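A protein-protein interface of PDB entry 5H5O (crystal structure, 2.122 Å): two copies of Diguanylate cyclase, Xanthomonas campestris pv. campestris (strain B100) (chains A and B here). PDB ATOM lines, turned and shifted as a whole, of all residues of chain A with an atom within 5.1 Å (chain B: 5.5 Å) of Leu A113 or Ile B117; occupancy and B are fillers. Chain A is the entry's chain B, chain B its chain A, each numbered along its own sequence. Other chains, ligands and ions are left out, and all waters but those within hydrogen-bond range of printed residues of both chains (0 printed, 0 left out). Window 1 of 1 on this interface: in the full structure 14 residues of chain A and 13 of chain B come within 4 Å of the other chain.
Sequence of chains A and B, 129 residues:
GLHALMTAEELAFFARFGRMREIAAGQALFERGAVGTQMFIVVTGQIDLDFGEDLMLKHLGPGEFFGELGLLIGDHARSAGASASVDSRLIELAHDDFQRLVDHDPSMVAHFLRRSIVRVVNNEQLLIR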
ATOM      1  N   LEU A  69     -28.490  14.878  18.550  1.00  0.00           N
ATOM      2  CA  LEU A  69     -29.589  14.660  19.485  1.00  0.00           C
ATOM      3  C   LEU A  69     -29.722  13.175  19.791  1.00  0.00           C
ATOM      4  O   LEU A  69     -29.890  12.793  20.943  1.00  0.00           O
ATOM      5  CB  LEU A  69     -30.921  15.182  18.935  1.00  0.00           C
ATOM      6  CG  LEU A  69     -31.016  16.652  18.519  1.00  0.00           C
ATOM      7  CD1 LEU A  69     -32.387  16.936  17.885  1.00  0.00           C
ATOM      8  CD2 LEU A  69     -30.749  17.590  19.694  1.00  0.00           C
ATOM      9  N   LEU A  72     -26.937  12.252  22.125  1.00  0.00           N
ATOM     10  CA  LEU A  72     -26.835  12.867  23.448  1.00  0.00           C
ATOM     11  C   LEU A  72     -28.036  12.587  24.357  1.00  0.00           C
ATOM     12  O   LEU A  72     -27.954  12.743  25.573  1.00  0.00           O
ATOM     13  CB  LEU A  72     -26.658  14.380  23.301  1.00  0.00           C
ATOM     14  CG  LEU A  72     -25.355  14.881  22.673  1.00  0.00           C
ATOM     15  CD1 LEU A  72     -25.460  16.348  22.279  1.00  0.00           C
ATOM     16  CD2 LEU A  72     -24.184  14.658  23.615  1.00  0.00           C
ATOM     17  N   ILE A  73     -29.148  12.182  23.762  1.00  0.00           N
ATOM     18  CA  ILE A  73     -30.384  11.985  24.498  1.00  0.00           C
ATOM     19  C   ILE A  73     -30.837  10.547  24.306  1.00  0.00           C
ATOM     20  O   ILE A  73     -31.152  10.136  23.198  1.00  0.00           O
ATOM     21  CB  ILE A  73     -31.463  12.932  23.977  1.00  0.00           C
ATOM     22  CG1 ILE A  73     -30.929  14.361  23.960  1.00  0.00           C
ATOM     23  CG2 ILE A  73     -32.723  12.869  24.837  1.00  0.00           C
ATOM     24  CD1 ILE A  73     -31.709  15.242  23.018  1.00  0.00           C
ATOM     25  N   PHE A  98     -17.943   8.928  21.644  1.00  0.00           N
ATOM     26  CA  PHE A  98     -18.138  10.245  22.221  1.00  0.00           C
ATOM     27  C   PHE A  98     -17.728  10.254  23.693  1.00  0.00           C
ATOM     28  O   PHE A  98     -17.109  11.215  24.164  1.00  0.00           O
ATOM     29  CB  PHE A  98     -19.588  10.733  22.043  1.00  0.00           C
ATOM     30  CG  PHE A  98     -19.854  12.073  22.669  1.00  0.00           C
ATOM     31  CD1 PHE A  98     -19.455  13.242  22.039  1.00  0.00           C
ATOM     32  CD2 PHE A  98     -20.487  12.159  23.909  1.00  0.00           C
ATOM     33  CE1 PHE A  98     -19.689  14.486  22.630  1.00  0.00           C
ATOM     34  CE2 PHE A  98     -20.724  13.391  24.501  1.00  0.00           C
ATOM     35  CZ  PHE A  98     -20.318  14.555  23.860  1.00  0.00           C
ATOM     36  N   VAL A 109     -14.874  19.090  23.623  1.00  0.00           N
ATOM     37  CA  VAL A 109     -16.268  18.642  23.645  1.00  0.00           C
ATOM     38  C   VAL A 109     -17.226  19.715  24.181  1.00  0.00           C
ATOM     39  O   VAL A 109     -18.316  19.903  23.647  1.00  0.00           O
ATOM     40  CB  VAL A 109     -16.422  17.323  24.438  1.00  0.00           C
ATOM     41  CG1 VAL A 109     -17.885  16.962  24.641  1.00  0.00           C
ATOM     42  CG2 VAL A 109     -15.697  16.200  23.716  1.00  0.00           C
ATOM     43  N   ALA A 110     -16.801  20.436  25.215  1.00  0.00           N
ATOM     44  CA  ALA A 110     -17.635  21.478  25.817  1.00  0.00           C
ATOM     45  C   ALA A 110     -17.917  22.573  24.796  1.00  0.00           C
ATOM     46  O   ALA A 110     -19.037  23.074  24.674  1.00  0.00           O
ATOM     47  CB  ALA A 110     -16.936  22.058  27.066  1.00  0.00           C
ATOM     48  N   HIS A 111     -16.877  22.932  24.045  1.00  0.00           N
ATOM     49  CA  HIS A 111     -17.001  23.951  23.011  1.00  0.00           C
ATOM     50  C   HIS A 111     -17.947  23.474  21.900  1.00  0.00           C
ATOM     51  O   HIS A 111     -18.825  24.227  21.433  1.00  0.00           O
ATOM     52  CB  HIS A 111     -15.614  24.322  22.470  1.00  0.00           C
ATOM     53  CG  HIS A 111     -15.633  25.445  21.481  1.00  0.00           C
ATOM     54  ND1 HIS A 111     -16.089  26.707  21.799  1.00  0.00           N
ATOM     55  CD2 HIS A 111     -15.252  25.495  20.183  1.00  0.00           C
ATOM     56  CE1 HIS A 111     -15.990  27.485  20.735  1.00  0.00           C
ATOM     57  NE2 HIS A 111     -15.488  26.775  19.741  1.00  0.00           N
ATOM     58  N   PHE A 112     -17.802  22.212  21.502  1.00  0.00           N
ATOM     59  CA  PHE A 112     -18.765  21.617  20.579  1.00  0.00           C
ATOM     60  C   PHE A 112     -20.202  21.633  21.122  1.00  0.00           C
ATOM     61  O   PHE A 112     -21.127  22.067  20.427  1.00  0.00           O
ATOM     62  CB  PHE A 112     -18.368  20.178  20.206  1.00  0.00           C
ATOM     63  CG  PHE A 112     -19.428  19.453  19.428  1.00  0.00           C
ATOM     64  CD1 PHE A 112     -19.689  19.795  18.098  1.00  0.00           C
ATOM     65  CD2 PHE A 112     -20.178  18.446  20.016  1.00  0.00           C
ATOM     66  CE1 PHE A 112     -20.682  19.151  17.380  1.00  0.00           C
ATOM     67  CE2 PHE A 112     -21.170  17.795  19.306  1.00  0.00           C
ATOM     68  CZ  PHE A 112     -21.427  18.142  17.984  1.00  0.00           C
ATOM     69  N   LEU A 113     -20.397  21.136  22.348  1.00  0.00           N
ATOM     70  CA  LEU A 113     -21.753  21.070  22.922  1.00  0.00           C
ATOM     71  C   LEU A 113     -22.393  22.452  22.936  1.00  0.00           C
ATOM     72  O   LEU A 113     -23.585  22.632  22.663  1.00  0.00           O
ATOM     73  CB  LEU A 113     -21.702  20.492  24.350  1.00  0.00           C
ATOM     74  CG  LEU A 113     -21.353  18.996  24.445  1.00  0.00           C
ATOM     75  CD1 LEU A 113     -21.254  18.532  25.910  1.00  0.00           C
ATOM     76  CD2 LEU A 113     -22.360  18.119  23.666  1.00  0.00           C
ATOM     77  N   ARG A 114     -21.580  23.440  23.261  1.00  0.00           N
ATOM     78  CA  ARG A 114     -22.030  24.816  23.310  1.00  0.00           C
ATOM     79  C   ARG A 114     -22.566  25.291  21.963  1.00  0.00           C
ATOM     80  O   ARG A 114     -23.664  25.857  21.879  1.00  0.00           O
ATOM     81  CB  ARG A 114     -20.862  25.686  23.750  1.00  0.00           C
ATOM     82  CG  ARG A 114     -21.234  27.069  24.176  1.00  0.00           C
ATOM     83  CD  ARG A 114     -20.112  27.636  25.015  1.00  0.00           C
ATOM     84  NE  ARG A 114     -20.239  29.074  25.174  1.00  0.00           N
ATOM     85  CZ  ARG A 114     -19.333  29.826  25.787  1.00  0.00           C
ATOM     86  NH1 ARG A 114     -18.240  29.260  26.291  1.00  0.00           N
ATOM     87  NH2 ARG A 114     -19.521  31.136  25.892  1.00  0.00           N
ATOM     88  N   ARG A 115     -21.775  25.080  20.914  1.00  0.00           N
ATOM     89  CA  ARG A 115     -22.211  25.431  19.577  1.00  0.00           C
ATOM     90  C   ARG A 115     -23.457  24.641  19.198  1.00  0.00           C
ATOM     91  O   ARG A 115     -24.346  25.179  18.537  1.00  0.00           O
ATOM     92  CB  ARG A 115     -21.095  25.202  18.549  1.00  0.00           C
ATOM     93  CG  ARG A 115     -19.870  26.055  18.768  1.00  0.00           C
ATOM     94  CD  ARG A 115     -19.173  26.366  17.437  1.00  0.00           C
ATOM     95  NE  ARG A 115     -19.235  25.236  16.508  1.00  0.00           N
ATOM     96  CZ  ARG A 115     -18.519  24.130  16.646  1.00  0.00           C
ATOM     97  NH1 ARG A 115     -17.697  24.000  17.688  1.00  0.00           N
ATOM     98  NH2 ARG A 115     -18.643  23.144  15.763  1.00  0.00           N
ATOM     99  N   SER A 116     -23.532  23.382  19.630  1.00  0.00           N
ATOM    100  CA  SER A 116     -24.716  22.558  19.369  1.00  0.00           C
ATOM    101  C   SER A 116     -25.971  23.218  19.900  1.00  0.00           C
ATOM    102  O   SER A 116     -26.989  23.284  19.211  1.00  0.00           O
ATOM    103  CB  SER A 116     -24.606  21.179  20.019  1.00  0.00           C
ATOM    104  OG  SER A 116     -23.767  20.325  19.276  1.00  0.00           O
ATOM    105  N   ILE A 117     -25.895  23.685  21.140  1.00  0.00           N
ATOM    106  CA  ILE A 117     -27.043  24.314  21.782  1.00  0.00           C
ATOM    107  C   ILE A 117     -27.496  25.532  20.992  1.00  0.00           C
ATOM    108  O   ILE A 117     -28.682  25.700  20.750  1.00  0.00           O
ATOM    109  CB  ILE A 117     -26.732  24.710  23.219  1.00  0.00           C
ATOM    110  CG1 ILE A 117     -26.598  23.452  24.064  1.00  0.00           C
ATOM    111  CG2 ILE A 117     -27.843  25.622  23.780  1.00  0.00           C
ATOM    112  CD1 ILE A 117     -26.187  23.719  25.512  1.00  0.00           C
ATOM    113  N   ALA B 110     -18.907  20.176  30.558  1.00  0.00           N
ATOM    114  CA  ALA B 110     -19.401  19.350  29.454  1.00  0.00           C
ATOM    115  C   ALA B 110     -20.550  18.483  29.931  1.00  0.00           C
ATOM    116  O   ALA B 110     -21.561  18.320  29.244  1.00  0.00           O
ATOM    117  CB  ALA B 110     -18.275  18.482  28.865  1.00  0.00           C
ATOM    118  N   HIS B 111     -20.387  17.919  31.125  1.00  0.00           N
ATOM    119  CA  HIS B 111     -21.433  17.089  31.703  1.00  0.00           C
ATOM    120  C   HIS B 111     -22.692  17.929  31.943  1.00  0.00           C
ATOM    121  O   HIS B 111     -23.830  17.504  31.643  1.00  0.00           O
ATOM    122  CB  HIS B 111     -20.926  16.438  32.990  1.00  0.00           C
ATOM    123  CG  HIS B 111     -21.824  15.365  33.517  1.00  0.00           C
ATOM    124  ND1 HIS B 111     -22.667  15.559  34.592  1.00  0.00           N
ATOM    125  CD2 HIS B 111     -22.011  14.084  33.120  1.00  0.00           C
ATOM    126  CE1 HIS B 111     -23.336  14.446  34.831  1.00  0.00           C
ATOM    127  NE2 HIS B 111     -22.956  13.534  33.952  1.00  0.00           N
ATOM    128  N   PHE B 112     -22.492  19.140  32.453  1.00  0.00           N
ATOM    129  CA  PHE B 112     -23.619  20.039  32.643  1.00  0.00           C
ATOM    130  C   PHE B 112     -24.278  20.395  31.307  1.00  0.00           C
ATOM    131  O   PHE B 112     -25.505  20.408  31.207  1.00  0.00           O
ATOM    132  CB  PHE B 112     -23.204  21.317  33.379  1.00  0.00           C
ATOM    133  CG  PHE B 112     -24.219  22.418  33.273  1.00  0.00           C
ATOM    134  CD1 PHE B 112     -25.374  22.397  34.060  1.00  0.00           C
ATOM    135  CD2 PHE B 112     -24.036  23.468  32.384  1.00  0.00           C
ATOM    136  CE1 PHE B 112     -26.326  23.401  33.959  1.00  0.00           C
ATOM    137  CE2 PHE B 112     -24.985  24.476  32.276  1.00  0.00           C
ATOM    138  CZ  PHE B 112     -26.135  24.443  33.063  1.00  0.00           C
ATOM    139  N   LEU B 113     -23.474  20.705  30.288  1.00  0.00           N
ATOM    140  CA  LEU B 113     -24.048  21.119  29.004  1.00  0.00           C
ATOM    141  C   LEU B 113     -24.840  19.983  28.363  1.00  0.00           C
ATOM    142  O   LEU B 113     -25.867  20.181  27.701  1.00  0.00           O
ATOM    143  CB  LEU B 113     -22.937  21.575  28.055  1.00  0.00           C
ATOM    144  CG  LEU B 113     -22.285  22.910  28.405  1.00  0.00           C
ATOM    145  CD1 LEU B 113     -21.075  23.193  27.497  1.00  0.00           C
ATOM    146  CD2 LEU B 113     -23.300  24.048  28.322  1.00  0.00           C
ATOM    147  N   ARG B 114     -24.326  18.781  28.539  1.00  0.00           N
ATOM    148  CA  ARG B 114     -24.988  17.585  28.072  1.00  0.00           C
ATOM    149  C   ARG B 114     -26.364  17.440  28.732  1.00  0.00           C
ATOM    150  O   ARG B 114     -27.371  17.227  28.046  1.00  0.00           O
ATOM    151  CB  ARG B 114     -24.099  16.395  28.408  1.00  0.00           C
ATOM    152  CG  ARG B 114     -24.538  15.099  27.834  1.00  0.00           C
ATOM    153  CD  ARG B 114     -23.344  14.181  27.748  1.00  0.00           C
ATOM    154  NE  ARG B 114     -23.752  12.830  27.406  1.00  0.00           N
ATOM    155  CZ  ARG B 114     -22.946  11.780  27.489  1.00  0.00           C
ATOM    156  NH1 ARG B 114     -21.690  11.942  27.901  1.00  0.00           N
ATOM    157  NH2 ARG B 114     -23.396  10.576  27.165  1.00  0.00           N
ATOM    158  N   ARG B 115     -26.404  17.557  30.061  1.00  0.00           N
ATOM    159  CA  ARG B 115     -27.666  17.519  30.775  1.00  0.00           C
ATOM    160  C   ARG B 115     -28.600  18.651  30.348  1.00  0.00           C
ATOM    161  O   ARG B 115     -29.802  18.459  30.290  1.00  0.00           O
ATOM    162  CB  ARG B 115     -27.462  17.540  32.294  1.00  0.00           C
ATOM    163  CG  ARG B 115     -26.741  16.327  32.840  1.00  0.00           C
ATOM    164  CD  ARG B 115     -27.239  15.975  34.259  1.00  0.00           C
ATOM    165  NE  ARG B 115     -27.616  17.154  35.040  1.00  0.00           N
ATOM    166  CZ  ARG B 115     -26.744  18.030  35.525  1.00  0.00           C
ATOM    167  NH1 ARG B 115     -25.445  17.865  35.288  1.00  0.00           N
ATOM    168  NH2 ARG B 115     -27.170  19.083  36.217  1.00  0.00           N
ATOM    169  N   SER B 116     -28.048  19.818  30.029  1.00  0.00           N
ATOM    170  CA  SER B 116     -28.862  20.923  29.528  1.00  0.00           C
ATOM    171  C   SER B 116     -29.594  20.579  28.228  1.00  0.00           C
ATOM    172  O   SER B 116     -30.799  20.821  28.094  1.00  0.00           O
ATOM    173  CB  SER B 116     -27.989  22.159  29.287  1.00  0.00           C
ATOM    174  OG  SER B 116     -27.592  22.737  30.511  1.00  0.00           O
ATOM    175  N   ILE B 117     -28.847  20.050  27.261  1.00  0.00           N
ATOM    176  CA  ILE B 117     -29.412  19.662  25.965  1.00  0.00           C
ATOM    177  C   ILE B 117     -30.608  18.716  26.112  1.00  0.00           C
ATOM    178  O   ILE B 117     -31.642  18.929  25.491  1.00  0.00           O
ATOM    179  CB  ILE B 117     -28.353  19.008  25.073  1.00  0.00           C
ATOM    180  CG1 ILE B 117     -27.380  20.072  24.582  1.00  0.00           C
ATOM    181  CG2 ILE B 117     -29.007  18.311  23.871  1.00  0.00           C
ATOM    182  CD1 ILE B 117     -26.040  19.509  24.132  1.00  0.00           C
ATOM    183  N   VAL B 118     -30.461  17.687  26.945  1.00  0.00           N
ATOM    184  CA  VAL B 118     -31.559  16.776  27.218  1.00  0.00           C
ATOM    185  C   VAL B 118     -32.776  17.539  27.750  1.00  0.00           C
ATOM    186  O   VAL B 118     -33.888  17.356  27.260  1.00  0.00           O
ATOM    187  CB  VAL B 118     -31.172  15.689  28.232  1.00  0.00           C
ATOM    188  CG1 VAL B 118     -32.383  14.821  28.539  1.00  0.00           C
ATOM    189  CG2 VAL B 118     -30.006  14.834  27.704  1.00  0.00           C
ATOM    190  N   ARG B 119     -32.557  18.415  28.730  1.00  0.00           N
ATOM    191  CA  ARG B 119     -33.650  19.178  29.318  1.00  0.00           C
ATOM    192  C   ARG B 119     -34.332  20.039  28.252  1.00  0.00           C
ATOM    193  O   ARG B 119     -35.554  20.049  28.142  1.00  0.00           O
ATOM    194  CB  ARG B 119     -33.145  20.044  30.483  1.00  0.00           C
ATOM    195  CG  ARG B 119     -34.235  20.486  31.468  1.00  0.00           C
ATOM    196  CD  ARG B 119     -33.836  21.748  32.246  1.00  0.00           C
ATOM    197  NE  ARG B 119     -33.733  22.904  31.358  1.00  0.00           N
ATOM    198  CZ  ARG B 119     -34.060  24.154  31.683  1.00  0.00           C
ATOM    199  NH1 ARG B 119     -34.518  24.447  32.899  1.00  0.00           N
ATOM    200  NH2 ARG B 119     -33.926  25.115  30.777  1.00  0.00           N
ATOM    201  N   VAL B 120     -33.531  20.726  27.447  1.00  0.00           N
ATOM    202  CA  VAL B 120     -34.037  21.686  26.473  1.00  0.00           C
ATOM    203  C   VAL B 120     -34.755  21.030  25.289  1.00  0.00           C
ATOM    204  O   VAL B 120     -35.732  21.573  24.771  1.00  0.00           O
ATOM    205  CB  VAL B 120     -32.916  22.632  26.001  1.00  0.00           C
ATOM    206  CG1 VAL B 120     -33.380  23.506  24.839  1.00  0.00           C
ATOM    207  CG2 VAL B 120     -32.470  23.504  27.169  1.00  0.00           C
ATOM    208  N   VAL B 121     -34.283  19.864  24.864  1.00  0.00           N
ATOM    209  CA  VAL B 121     -34.976  19.130  23.811  1.00  0.00           C
ATOM    210  C   VAL B 121     -36.319  18.634  24.346  1.00  0.00           C
ATOM    211  O   VAL B 121     -37.293  18.503  23.598  1.00  0.00           O
ATOM    212  CB  VAL B 121     -34.108  17.987  23.244  1.00  0.00           C
ATOM    213  CG1 VAL B 121     -34.933  17.037  22.372  1.00  0.00           C
ATOM    214  CG2 VAL B 121     -32.954  18.581  22.452  1.00  0.00           C
ATOM    215  N   ASN B 122     -36.373  18.422  25.656  1.00  0.00           N
ATOM    216  CA  ASN B 122     -37.606  18.033  26.324  1.00  0.00           C
ATOM    217  C   ASN B 122     -38.357  19.228  26.920  1.00  0.00           C
ATOM    218  O   ASN B 122     -39.095  19.075  27.891  1.00  0.00           O
ATOM    219  CB  ASN B 122     -37.319  17.003  27.421  1.00  0.00           C
ATOM    220  CG  ASN B 122     -36.863  15.668  26.865  1.00  0.00           C
ATOM    221  OD1 ASN B 122     -37.069  15.369  25.689  1.00  0.00           O
ATOM    222  ND2 ASN B 122     -36.240  14.857  27.709  1.00  0.00           N
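Ala A110 touches Leu B113, and with the chains exchanged Leu A113 touches Ala B110. Leu A113 touches Ile B117, but with the chains exchanged Ile A117 does not touch Leu B113 (4.04 Å). Ile A117 touches its own counterpart, Ile B117. 8 positions are printed for both chains. Of the 10 pairs that touch across the chains among the printed residues, 3 have their exchanged pair printed and touching as well.
CG2 of Val B121 touches CD2 of Leu A69, at 3.7 Å. Ile B117 touches Leu A72. Leu A72 touches Val B118 (O to CG2, 3.6 Å). Val B118 touches Ile A73 (CG2 to CG1, 3.9 Å). CD1 of Ile A73 touches CG2 of Val B121 (3.6 Å). Phe A98 touches Arg B114. CD1 of Leu B113 touches O of Ala A110, 3.5 Å away. O of Ala B110 touches CD1 of Leu A113, at 3.4 Å. CD2 of Leu A113 touches CD1 of Ile B117, 3.96 Å away. CG1 of Ile A117 touches CG1 of Ile B117 (3.5 Å).
Of the printed residues of chain B, Leu A69 touches Val B121 (3.7 Å). Of the printed residues of chain B, Ile A73 touches Val B118 (3.9 Å) and Val B121 (3.6 Å). Printed residues of chain B within 4 Å of Ala A110: Leu B113 (3.5 Å). Leu A113 touches two residues of chain B. Of chain A, only Leu A72, Leu A113 and Ile A117 come within 4 Å of Ile B117. The nearest printed residue of chain B that does not touch Leu A113 is Arg B114 (4.1 Å). The nearest printed residue of chain B that does not touch Ile A117 is Leu B113 (4.04 Å).
The backbone carbonyl oxygen of Val B118 lies close to the side-chain amide nitrogen of Asn B122 (3.5 Å).
Of the 13 printed residues of chain B, 6 touch a printed residue of chain A. Hydrophobic or aromatic side chains of chain A within 4 Å of the printed part of chain B: Leu A69, Leu A72, Ile A73, Phe A98, Leu A113 and Ile A117. Among the printed residues, 10 pairs touch across the chains.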
